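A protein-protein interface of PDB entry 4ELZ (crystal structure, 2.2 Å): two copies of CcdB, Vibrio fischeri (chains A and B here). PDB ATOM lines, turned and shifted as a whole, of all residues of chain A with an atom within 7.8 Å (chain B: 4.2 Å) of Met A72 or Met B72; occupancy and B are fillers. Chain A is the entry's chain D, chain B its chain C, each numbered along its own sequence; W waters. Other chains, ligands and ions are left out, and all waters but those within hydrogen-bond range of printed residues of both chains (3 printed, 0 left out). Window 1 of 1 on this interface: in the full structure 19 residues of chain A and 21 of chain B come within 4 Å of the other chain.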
ATOM      1  N   VAL A  22       8.105 -27.253  31.107  1.00  0.00           N
ATOM      2  CA  VAL A  22       9.117 -27.220  30.064  1.00  0.00           C
ATOM      3  C   VAL A  22       8.791 -26.135  29.034  1.00  0.00           C
ATOM      4  O   VAL A  22       7.651 -25.995  28.604  1.00  0.00           O
ATOM      5  CB  VAL A  22       9.289 -28.609  29.401  1.00  0.00           C
ATOM      6  CG1 VAL A  22       7.968 -29.126  28.884  1.00  0.00           C
ATOM      7  CG2 VAL A  22      10.324 -28.561  28.283  1.00  0.00           C
ATOM      8  N   VAL A  24       8.718 -24.850  25.409  1.00  0.00           N
ATOM      9  CA  VAL A  24       8.694 -25.529  24.107  1.00  0.00           C
ATOM     10  C   VAL A  24       8.721 -24.562  22.920  1.00  0.00           C
ATOM     11  O   VAL A  24       8.634 -24.970  21.749  1.00  0.00           O
ATOM     12  CB  VAL A  24       7.487 -26.488  23.981  1.00  0.00           C
ATOM     13  CG1 VAL A  24       7.572 -27.581  25.060  1.00  0.00           C
ATOM     14  CG2 VAL A  24       6.160 -25.708  24.063  1.00  0.00           C
ATOM     15  N   THR A  34       6.472 -13.525  26.214  1.00  0.00           N
ATOM     16  CA  THR A  34       5.729 -14.699  26.669  1.00  0.00           C
ATOM     17  C   THR A  34       6.427 -15.986  26.239  1.00  0.00           C
ATOM     18  O   THR A  34       7.263 -15.976  25.338  1.00  0.00           O
ATOM     19  CB  THR A  34       4.288 -14.735  26.105  1.00  0.00           C
ATOM     20  OG1 THR A  34       4.333 -14.617  24.673  1.00  0.00           O
ATOM     21  CG2 THR A  34       3.426 -13.599  26.704  1.00  0.00           C
ATOM     22  N   ARG A  35       6.069 -17.093  26.889  1.00  0.00           N
ATOM     23  CA  ARG A  35       6.654 -18.391  26.602  1.00  0.00           C
ATOM     24  C   ARG A  35       5.559 -19.448  26.587  1.00  0.00           C
ATOM     25  O   ARG A  35       4.731 -19.529  27.487  1.00  0.00           O
ATOM     26  CB  ARG A  35       7.708 -18.752  27.657  1.00  0.00           C
ATOM     27  CG  ARG A  35       8.995 -17.904  27.590  1.00  0.00           C
ATOM     28  CD  ARG A  35       9.742 -18.108  26.261  1.00  0.00           C
ATOM     29  NE  ARG A  35      11.026 -17.400  26.236  1.00  0.00           N
ATOM     30  CZ  ARG A  35      11.187 -16.148  25.808  1.00  0.00           C
ATOM     31  NH1 ARG A  35      10.145 -15.443  25.365  1.00  0.00           N
ATOM     32  NH2 ARG A  35      12.388 -15.589  25.823  1.00  0.00           N
ATOM     33  N   LEU A  36       5.544 -20.262  25.551  1.00  0.00           N
ATOM     34  CA  LEU A  36       4.643 -21.389  25.532  1.00  0.00           C
ATOM     35  C   LEU A  36       5.288 -22.508  26.341  1.00  0.00           C
ATOM     36  O   LEU A  36       6.379 -22.966  26.004  1.00  0.00           O
ATOM     37  CB  LEU A  36       4.431 -21.830  24.085  1.00  0.00           C
ATOM     38  CG  LEU A  36       3.440 -22.972  23.887  1.00  0.00           C
ATOM     39  CD1 LEU A  36       2.042 -22.534  24.317  1.00  0.00           C
ATOM     40  CD2 LEU A  36       3.466 -23.435  22.423  1.00  0.00           C
ATOM     41  N   VAL A  37       4.638 -22.949  27.412  1.00  0.00           N
ATOM     42  CA  VAL A  37       5.241 -23.979  28.269  1.00  0.00           C
ATOM     43  C   VAL A  37       4.258 -25.123  28.507  1.00  0.00           C
ATOM     44  O   VAL A  37       3.039 -24.948  28.345  1.00  0.00           O
ATOM     45  CB  VAL A  37       5.682 -23.410  29.656  1.00  0.00           C
ATOM     46  CG1 VAL A  37       6.622 -22.227  29.489  1.00  0.00           C
ATOM     47  CG2 VAL A  37       4.450 -23.011  30.493  1.00  0.00           C
ATOM     48  N   ILE A  38       4.787 -26.279  28.906  1.00  0.00           N
ATOM     49  CA  ILE A  38       3.968 -27.442  29.256  1.00  0.00           C
ATOM     50  C   ILE A  38       4.268 -27.896  30.676  1.00  0.00           C
ATOM     51  O   ILE A  38       5.425 -28.142  31.023  1.00  0.00           O
ATOM     52  CB  ILE A  38       4.218 -28.645  28.304  1.00  0.00           C
ATOM     53  CG1 ILE A  38       3.929 -28.261  26.855  1.00  0.00           C
ATOM     54  CG2 ILE A  38       3.338 -29.834  28.692  1.00  0.00           C
ATOM     55  CD1 ILE A  38       4.192 -29.416  25.851  1.00  0.00           C
ATOM     56  N   PRO A  39       3.222 -28.029  31.499  1.00  0.00           N
ATOM     57  CA  PRO A  39       3.366 -28.466  32.891  1.00  0.00           C
ATOM     58  C   PRO A  39       3.762 -29.931  32.985  1.00  0.00           C
ATOM     59  O   PRO A  39       3.334 -30.725  32.155  1.00  0.00           O
ATOM     60  CB  PRO A  39       1.947 -28.314  33.460  1.00  0.00           C
ATOM     61  CG  PRO A  39       1.192 -27.496  32.469  1.00  0.00           C
ATOM     62  CD  PRO A  39       1.819 -27.743  31.146  1.00  0.00           C
ATOM     63  N   MET A  67       4.002 -35.451  31.247  1.00  0.00           N
ATOM     64  CA  MET A  67       3.941 -34.136  30.643  1.00  0.00           C
ATOM     65  C   MET A  67       2.521 -33.871  30.151  1.00  0.00           C
ATOM     66  O   MET A  67       2.055 -34.500  29.202  1.00  0.00           O
ATOM     67  CB  MET A  67       4.937 -34.074  29.488  1.00  0.00           C
ATOM     68  CG  MET A  67       5.013 -32.734  28.823  1.00  0.00           C
ATOM     69  SD  MET A  67       6.329 -32.645  27.609  1.00  0.00           S
ATOM     70  CE  MET A  67       7.690 -33.204  28.628  1.00  0.00           C
ATOM     71  N   LEU A  68       1.830 -32.951  30.804  1.00  0.00           N
ATOM     72  CA  LEU A  68       0.432 -32.678  30.482  1.00  0.00           C
ATOM     73  C   LEU A  68       0.303 -31.727  29.306  1.00  0.00           C
ATOM     74  O   LEU A  68      -0.002 -30.539  29.486  1.00  0.00           O
ATOM     75  CB  LEU A  68      -0.271 -32.071  31.690  1.00  0.00           C
ATOM     76  CG  LEU A  68      -0.329 -32.971  32.913  1.00  0.00           C
ATOM     77  CD1 LEU A  68      -0.707 -32.157  34.124  1.00  0.00           C
ATOM     78  CD2 LEU A  68      -1.352 -34.055  32.665  1.00  0.00           C
ATOM     79  N   THR A  69       0.518 -32.261  28.107  1.00  0.00           N
ATOM     80  CA  THR A  69       0.476 -31.497  26.866  1.00  0.00           C
ATOM     81  C   THR A  69      -0.821 -30.696  26.712  1.00  0.00           C
ATOM     82  O   THR A  69      -0.805 -29.554  26.245  1.00  0.00           O
ATOM     83  CB  THR A  69       0.648 -32.444  25.659  1.00  0.00           C
ATOM     84  OG1 THR A  69       1.808 -33.257  25.867  1.00  0.00           O
ATOM     85  CG2 THR A  69       0.815 -31.667  24.359  1.00  0.00           C
ATOM     86  N   GLN A  70      -1.936 -31.285  27.133  1.00  0.00           N
ATOM     87  CA  GLN A  70      -3.240 -30.645  26.973  1.00  0.00           C
ATOM     88  C   GLN A  70      -3.410 -29.405  27.851  1.00  0.00           C
ATOM     89  O   GLN A  70      -4.350 -28.630  27.655  1.00  0.00           O
ATOM     90  CB  GLN A  70      -4.388 -31.642  27.217  1.00  0.00           C
ATOM     91  CG  GLN A  70      -4.751 -31.877  28.680  1.00  0.00           C
ATOM     92  CD  GLN A  70      -4.039 -33.071  29.283  1.00  0.00           C
ATOM     93  OE1 GLN A  70      -3.012 -33.524  28.773  1.00  0.00           O
ATOM     94  NE2 GLN A  70      -4.588 -33.592  30.376  1.00  0.00           N
ATOM     95  N   GLN A  71      -2.496 -29.210  28.798  1.00  0.00           N
ATOM     96  CA  GLN A  71      -2.521 -28.032  29.665  1.00  0.00           C
ATOM     97  C   GLN A  71      -1.458 -27.013  29.257  1.00  0.00           C
ATOM     98  O   GLN A  71      -1.155 -26.080  30.008  1.00  0.00           O
ATOM     99  CB  GLN A  71      -2.361 -28.438  31.131  1.00  0.00           C
ATOM    100  CG  GLN A  71      -3.200 -29.654  31.480  1.00  0.00           C
ATOM    101  CD  GLN A  71      -3.855 -29.558  32.832  1.00  0.00           C
ATOM    102  OE1 GLN A  71      -3.548 -28.666  33.626  1.00  0.00           O
ATOM    103  NE2 GLN A  71      -4.768 -30.483  33.107  1.00  0.00           N
ATOM    104  N   MET A  72      -0.899 -27.211  28.064  1.00  0.00           N
ATOM    105  CA  MET A  72       0.013 -26.263  27.440  1.00  0.00           C
ATOM    106  C   MET A  72      -0.576 -24.872  27.490  1.00  0.00           C
ATOM    107  O   MET A  72      -1.768 -24.696  27.248  1.00  0.00           O
ATOM    108  CB  MET A  72       0.194 -26.630  25.965  1.00  0.00           C
ATOM    109  CG  MET A  72       1.423 -26.040  25.312  1.00  0.00           C
ATOM    110  SD  MET A  72       1.646 -26.728  23.656  1.00  0.00           S
ATOM    111  CE  MET A  72       0.093 -26.223  22.966  1.00  0.00           C
ATOM    112  N   THR A  73       0.262 -23.880  27.763  1.00  0.00           N
ATOM    113  CA  THR A  73      -0.221 -22.511  27.908  1.00  0.00           C
ATOM    114  C   THR A  73       0.921 -21.501  27.824  1.00  0.00           C
ATOM    115  O   THR A  73       2.067 -21.800  28.154  1.00  0.00           O
ATOM    116  CB  THR A  73      -0.983 -22.313  29.250  1.00  0.00           C
ATOM    117  OG1 THR A  73      -1.529 -20.986  29.316  1.00  0.00           O
ATOM    118  CG2 THR A  73      -0.059 -22.531  30.442  1.00  0.00           C
ATOM    119  N   SER A  74       0.599 -20.300  27.367  1.00  0.00           N
ATOM    120  CA  SER A  74       1.588 -19.241  27.303  1.00  0.00           C
ATOM    121  C   SER A  74       1.619 -18.539  28.644  1.00  0.00           C
ATOM    122  O   SER A  74       0.574 -18.316  29.250  1.00  0.00           O
ATOM    123  CB  SER A  74       1.252 -18.252  26.195  1.00  0.00           C
ATOM    124  OG  SER A  74      -0.078 -17.789  26.340  1.00  0.00           O
ATOM    125  N   VAL A  75       2.836 -18.232  29.106  1.00  0.00           N
ATOM    126  CA  VAL A  75       3.074 -17.551  30.388  1.00  0.00           C
ATOM    127  C   VAL A  75       4.027 -16.366  30.197  1.00  0.00           C
ATOM    128  O   VAL A  75       4.799 -16.335  29.226  1.00  0.00           O
ATOM    129  CB  VAL A  75       3.721 -18.508  31.416  1.00  0.00           C
ATOM    130  CG1 VAL A  75       2.769 -19.634  31.761  1.00  0.00           C
ATOM    131  CG2 VAL A  75       5.074 -19.047  30.889  1.00  0.00           C
ATOM    132  N   ILE A  94       8.225 -34.853  22.489  1.00  0.00           N
ATOM    133  CA  ILE A  94       7.488 -33.648  22.857  1.00  0.00           C
ATOM    134  C   ILE A  94       6.783 -33.059  21.649  1.00  0.00           C
ATOM    135  O   ILE A  94       5.583 -32.768  21.693  1.00  0.00           O
ATOM    136  CB  ILE A  94       8.414 -32.609  23.550  1.00  0.00           C
ATOM    137  CG1 ILE A  94       8.862 -33.158  24.910  1.00  0.00           C
ATOM    138  CG2 ILE A  94       7.707 -31.267  23.738  1.00  0.00           C
ATOM    139  CD1 ILE A  94       9.971 -32.348  25.608  1.00  0.00           C
ATOM    140  N   ALA A  97       3.882 -35.321  20.724  1.00  0.00           N
ATOM    141  CA  ALA A  97       2.721 -35.128  21.604  1.00  0.00           C
ATOM    142  C   ALA A  97       1.943 -33.874  21.235  1.00  0.00           C
ATOM    143  O   ALA A  97       0.708 -33.886  21.199  1.00  0.00           O
ATOM    144  CB  ALA A  97       3.150 -35.059  23.044  1.00  0.00           C
ATOM    145  N   ILE A  98       2.665 -32.791  20.956  1.00  0.00           N
ATOM    146  CA  ILE A  98       2.035 -31.543  20.532  1.00  0.00           C
ATOM    147  C   ILE A  98       1.283 -31.720  19.228  1.00  0.00           C
ATOM    148  O   ILE A  98       0.171 -31.210  19.078  1.00  0.00           O
ATOM    149  CB  ILE A  98       3.061 -30.393  20.396  1.00  0.00           C
ATOM    150  CG1 ILE A  98       3.510 -29.930  21.788  1.00  0.00           C
ATOM    151  CG2 ILE A  98       2.433 -29.217  19.636  1.00  0.00           C
ATOM    152  CD1 ILE A  98       4.673 -28.948  21.781  1.00  0.00           C
ATOM    153  N   LEU A 101      -2.022 -33.500  19.865  1.00  0.00           N
ATOM    154  CA  LEU A 101      -3.030 -32.582  20.386  1.00  0.00           C
ATOM    155  C   LEU A 101      -3.684 -31.772  19.262  1.00  0.00           C
ATOM    156  O   LEU A 101      -4.887 -31.500  19.294  1.00  0.00           O
ATOM    157  CB  LEU A 101      -2.396 -31.638  21.438  1.00  0.00           C
ATOM    158  CG  LEU A 101      -3.317 -30.670  22.197  1.00  0.00           C
ATOM    159  CD1 LEU A 101      -4.406 -31.439  22.917  1.00  0.00           C
ATOM    160  CD2 LEU A 101      -2.537 -29.806  23.194  1.00  0.00           C
ATOM    161  N   ILE A 102      -2.902 -31.409  18.252  1.00  0.00           N
ATOM    162  CA  ILE A 102      -3.363 -30.473  17.220  1.00  0.00           C
ATOM    163  C   ILE A 102      -3.742 -31.090  15.869  1.00  0.00           C
ATOM    164  O   ILE A 102      -4.776 -30.745  15.301  1.00  0.00           O
ATOM    165  CB  ILE A 102      -2.325 -29.343  17.021  1.00  0.00           C
ATOM    166  CG1 ILE A 102      -2.274 -28.475  18.278  1.00  0.00           C
ATOM    167  CG2 ILE A 102      -2.675 -28.477  15.839  1.00  0.00           C
ATOM    168  CD1 ILE A 102      -1.291 -27.354  18.190  1.00  0.00           C
ATOM    169  N   VAL B  24      -8.283 -24.912  18.558  1.00  0.00           N
ATOM    170  CA  VAL B  24      -7.382 -25.525  17.580  1.00  0.00           C
ATOM    171  C   VAL B  24      -7.052 -26.985  17.932  1.00  0.00           C
ATOM    172  O   VAL B  24      -6.216 -27.619  17.292  1.00  0.00           O
ATOM    173  CB  VAL B  24      -6.080 -24.706  17.399  1.00  0.00           C
ATOM    174  CG1 VAL B  24      -6.410 -23.274  16.925  1.00  0.00           C
ATOM    175  CG2 VAL B  24      -5.275 -24.682  18.690  1.00  0.00           C
ATOM    176  N   LEU B  36      -7.357 -26.325  23.872  1.00  0.00           N
ATOM    177  CA  LEU B  36      -6.321 -25.417  23.409  1.00  0.00           C
ATOM    178  C   LEU B  36      -6.938 -24.361  22.503  1.00  0.00           C
ATOM    179  O   LEU B  36      -7.521 -24.710  21.480  1.00  0.00           O
ATOM    180  CB  LEU B  36      -5.325 -26.216  22.577  1.00  0.00           C
ATOM    181  CG  LEU B  36      -3.982 -25.551  22.309  1.00  0.00           C
ATOM    182  CD1 LEU B  36      -3.341 -25.187  23.629  1.00  0.00           C
ATOM    183  CD2 LEU B  36      -3.083 -26.510  21.512  1.00  0.00           C
ATOM    184  N   VAL B  37      -6.803 -23.081  22.854  1.00  0.00           N
ATOM    185  CA  VAL B  37      -7.416 -22.006  22.052  1.00  0.00           C
ATOM    186  C   VAL B  37      -6.427 -20.901  21.723  1.00  0.00           C
ATOM    187  O   VAL B  37      -5.409 -20.731  22.407  1.00  0.00           O
ATOM    188  CB  VAL B  37      -8.667 -21.377  22.733  1.00  0.00           C
ATOM    189  CG1 VAL B  37      -9.661 -22.453  23.092  1.00  0.00           C
ATOM    190  CG2 VAL B  37      -8.278 -20.582  23.990  1.00  0.00           C
ATOM    191  N   ILE B  38      -6.708 -20.172  20.646  1.00  0.00           N
ATOM    192  CA  ILE B  38      -5.910 -19.004  20.284  1.00  0.00           C
ATOM    193  C   ILE B  38      -6.824 -17.791  20.234  1.00  0.00           C
ATOM    194  O   ILE B  38      -7.851 -17.812  19.542  1.00  0.00           O
ATOM    195  CB  ILE B  38      -5.262 -19.158  18.905  1.00  0.00           C
ATOM    196  CG1 ILE B  38      -4.325 -20.360  18.878  1.00  0.00           C
ATOM    197  CG2 ILE B  38      -4.497 -17.885  18.532  1.00  0.00           C
ATOM    198  CD1 ILE B  38      -3.650 -20.537  17.539  1.00  0.00           C
ATOM    199  N   LEU B  68      -3.311 -14.315  17.671  1.00  0.00           N
ATOM    200  CA  LEU B  68      -2.163 -14.240  18.556  1.00  0.00           C
ATOM    201  C   LEU B  68      -1.702 -15.622  18.980  1.00  0.00           C
ATOM    202  O   LEU B  68      -1.892 -16.030  20.122  1.00  0.00           O
ATOM    203  CB  LEU B  68      -2.512 -13.408  19.781  1.00  0.00           C
ATOM    204  CG  LEU B  68      -2.800 -11.958  19.422  1.00  0.00           C
ATOM    205  CD1 LEU B  68      -3.576 -11.344  20.555  1.00  0.00           C
ATOM    206  CD2 LEU B  68      -1.487 -11.211  19.181  1.00  0.00           C
ATOM    207  N   THR B  69      -1.095 -16.335  18.040  1.00  0.00           N
ATOM    208  CA  THR B  69      -0.634 -17.691  18.265  1.00  0.00           C
ATOM    209  C   THR B  69       0.225 -17.835  19.515  1.00  0.00           C
ATOM    210  O   THR B  69       0.075 -18.795  20.263  1.00  0.00           O
ATOM    211  CB  THR B  69       0.163 -18.156  17.053  1.00  0.00           C
ATOM    212  OG1 THR B  69      -0.609 -17.875  15.877  1.00  0.00           O
ATOM    213  CG2 THR B  69       0.454 -19.639  17.139  1.00  0.00           C
ATOM    214  N   GLN B  70       1.103 -16.867  19.759  1.00  0.00           N
ATOM    215  CA  GLN B  70       1.997 -16.938  20.904  1.00  0.00           C
ATOM    216  C   GLN B  70       1.263 -16.826  22.238  1.00  0.00           C
ATOM    217  O   GLN B  70       1.865 -17.044  23.293  1.00  0.00           O
ATOM    218  CB  GLN B  70       3.121 -15.891  20.807  1.00  0.00           C
ATOM    219  CG  GLN B  70       2.718 -14.455  21.109  1.00  0.00           C
ATOM    220  CD  GLN B  70       2.063 -13.768  19.928  1.00  0.00           C
ATOM    221  OE1 GLN B  70       1.539 -14.423  19.020  1.00  0.00           O
ATOM    222  NE2 GLN B  70       2.102 -12.441  19.923  1.00  0.00           N
ATOM    223  N   GLN B  71      -0.033 -16.509  22.189  1.00  0.00           N
ATOM    224  CA  GLN B  71      -0.836 -16.418  23.407  1.00  0.00           C
ATOM    225  C   GLN B  71      -1.850 -17.528  23.481  1.00  0.00           C
ATOM    226  O   GLN B  71      -2.858 -17.403  24.176  1.00  0.00           O
ATOM    227  CB  GLN B  71      -1.513 -15.055  23.513  1.00  0.00           C
ATOM    228  CG  GLN B  71      -0.489 -14.028  23.984  1.00  0.00           C
ATOM    229  CD  GLN B  71      -1.003 -12.612  24.044  1.00  0.00           C
ATOM    230  OE1 GLN B  71      -2.210 -12.367  24.114  1.00  0.00           O
ATOM    231  NE2 GLN B  71      -0.075 -11.656  24.025  1.00  0.00           N
ATOM    232  N   MET B  72      -1.588 -18.612  22.750  1.00  0.00           N
ATOM    233  CA  MET B  72      -2.455 -19.779  22.818  1.00  0.00           C
ATOM    234  C   MET B  72      -2.440 -20.348  24.232  1.00  0.00           C
ATOM    235  O   MET B  72      -1.436 -20.260  24.940  1.00  0.00           O
ATOM    236  CB  MET B  72      -2.037 -20.842  21.801  1.00  0.00           C
ATOM    237  CG  MET B  72      -1.123 -21.908  22.341  1.00  0.00           C
ATOM    238  SD  MET B  72      -0.309 -22.790  20.989  1.00  0.00           S
ATOM    239  CE  MET B  72      -1.720 -23.480  20.163  1.00  0.00           C
ATOM    240  N   THR B  73      -3.560 -20.922  24.650  1.00  0.00           N
ATOM    241  CA  THR B  73      -3.647 -21.446  26.003  1.00  0.00           C
ATOM    242  C   THR B  73      -4.746 -22.497  26.121  1.00  0.00           C
ATOM    243  O   THR B  73      -5.662 -22.562  25.305  1.00  0.00           O
ATOM    244  CB  THR B  73      -3.832 -20.300  27.062  1.00  0.00           C
ATOM    245  OG1 THR B  73      -3.891 -20.847  28.392  1.00  0.00           O
ATOM    246  CG2 THR B  73      -5.091 -19.505  26.810  1.00  0.00           C
ATOM    247  N   SER B  74      -4.621 -23.331  27.142  1.00  0.00           N
ATOM    248  CA  SER B  74      -5.604 -24.340  27.461  1.00  0.00           C
ATOM    249  C   SER B  74      -6.663 -23.691  28.350  1.00  0.00           C
ATOM    250  O   SER B  74      -6.326 -23.044  29.341  1.00  0.00           O
ATOM    251  CB  SER B  74      -4.895 -25.483  28.200  1.00  0.00           C
ATOM    252  OG  SER B  74      -5.804 -26.366  28.830  1.00  0.00           O
ATOM    253  N   ILE B  98       1.355 -22.127  14.227  1.00  0.00           N
ATOM    254  CA  ILE B  98       1.748 -22.942  15.362  1.00  0.00           C
ATOM    255  C   ILE B  98       3.117 -23.609  15.188  1.00  0.00           C
ATOM    256  O   ILE B  98       3.946 -23.558  16.101  1.00  0.00           O
ATOM    257  CB  ILE B  98       0.660 -23.986  15.658  1.00  0.00           C
ATOM    258  CG1 ILE B  98      -0.575 -23.269  16.210  1.00  0.00           C
ATOM    259  CG2 ILE B  98       1.174 -25.031  16.638  1.00  0.00           C
ATOM    260  CD1 ILE B  98      -1.846 -24.086  16.143  1.00  0.00           C
HETATM  261  O   HOH W   1      -4.893 -26.495  32.048  1.00  0.00           O
HETATM  262  O   HOH W   2       4.551 -17.041  23.760  1.00  0.00           O
HETATM  263  O   HOH W   3      -3.827 -22.393  30.742  1.00  0.00           O
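The backbone carbonyl oxygen (O) of Met B72 lies within hydrogen-bond range of the side-chain hydroxyl (OG) of Ser A74 (3.1 Å). N of Ser B74 is in hydrogen-bond range of O of Met A72, 3.2 Å away. The side-chain hydroxyl (OG1) of Thr B73 sits at hydrogen-bond distance from the side-chain hydroxyl (OG1) of Thr A73 (2.5 Å). OG of Ser B74 sits at hydrogen-bond distance from O of Gln A70 (2.9 Å).
Gln A70 touches Ser B74, and with the chains exchanged Ser A74 touches Gln B70. Gln A71 touches Ser B74, and with the chains exchanged Ser A74 touches Gln B71. Met A72 touches Ser B74, and with the chains exchanged Ser A74 touches Met B72. Thr A73 touches its own counterpart, Thr B73. Positions printed for both chains: 24, 36, 37, 38, 68, 69, 70, 71, 72, 73, 74 and 98. Of the 17 pairs that touch across the chains among the printed residues, 12 have their exchanged pair printed and touching as well.
Of the 22 printed residues of chain A, 9 touch a printed residue of chain B. Along chain A the printed residues that touch a printed residue of chain B span positions 34 to 102. Among the printed residues, 17 pairs touch across the chains.
Printed residues of chain B within 4 Å of Met A72: Leu B36 (3.5 Å), Met B72 (3.98 Å), Thr B73 (3.9 Å) and Ser B74 (3.2 Å). Of the printed residues of chain A, Met B72 touches Leu A36, Met A72, Thr A73 and Ser A74. Of the printed residues of chain B, Leu A36 touches Met B72 (3.8 Å). Of the printed residues of chain B, Thr A73 touches Met B72 (3.9 Å) and Thr B73 (2.5 Å). Printed residues of chain B within 4 Å of Ser A74: Gln B70 (3.2 Å), Gln B71 (3.3 Å) and Met B72 (3.1 Å). Of the printed residues of chain A, Thr B73 touches Met A72 and Thr A73. The nearest printed residue of chain B that does not touch Met A72 is Ile B98 (6.5 Å). The nearest printed residue of chain B that does not touch Ser A74 is Thr B73 (4.4 Å).
Water W2 lies within hydrogen-bond range of OG1 of Thr A34 (2.6 Å), O of Gln B70 (2.7 Å) and N of Arg A35 (3.5 Å). Water W3 lies within hydrogen-bond range of the side-chain hydroxyl of Thr B73, the backbone carbonyl oxygen of Ser B74 and the side-chain hydroxyl of Thr A73. Water W1 lies within hydrogen-bond range of OE1 of Gln A71 (3.0 Å) and OG of Ser B74 (3.3 Å).
The backbone NH (N) of Val B37 sits at hydrogen-bond distance from the backbone carbonyl oxygen (O) of Thr B73, 2.8 Å away. O of Leu B36 is in hydrogen-bond range of N of Val B24. The backbone NH of Val A37 lies within hydrogen-bond range of the backbone carbonyl oxygen of Thr A73, at 2.9 Å. N of Val A24 lies within hydrogen-bond range of O of Leu A36 (3.1 Å).
Gln B70 touches Thr A34. Leu A36 touches Met B72. Gln A71 touches Ser B74. Met A72 touches Leu B36 (CE to CD2, 3.5 Å). Met A72 touches Met B72. Gln B70 touches Ser A74. Gln B71 touches Ser A74. Leu A101 touches Leu B36. Ile A102 touches Val B24. Ile A102 touches Ile B98 (CD1 to CG2, 3.7 Å).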
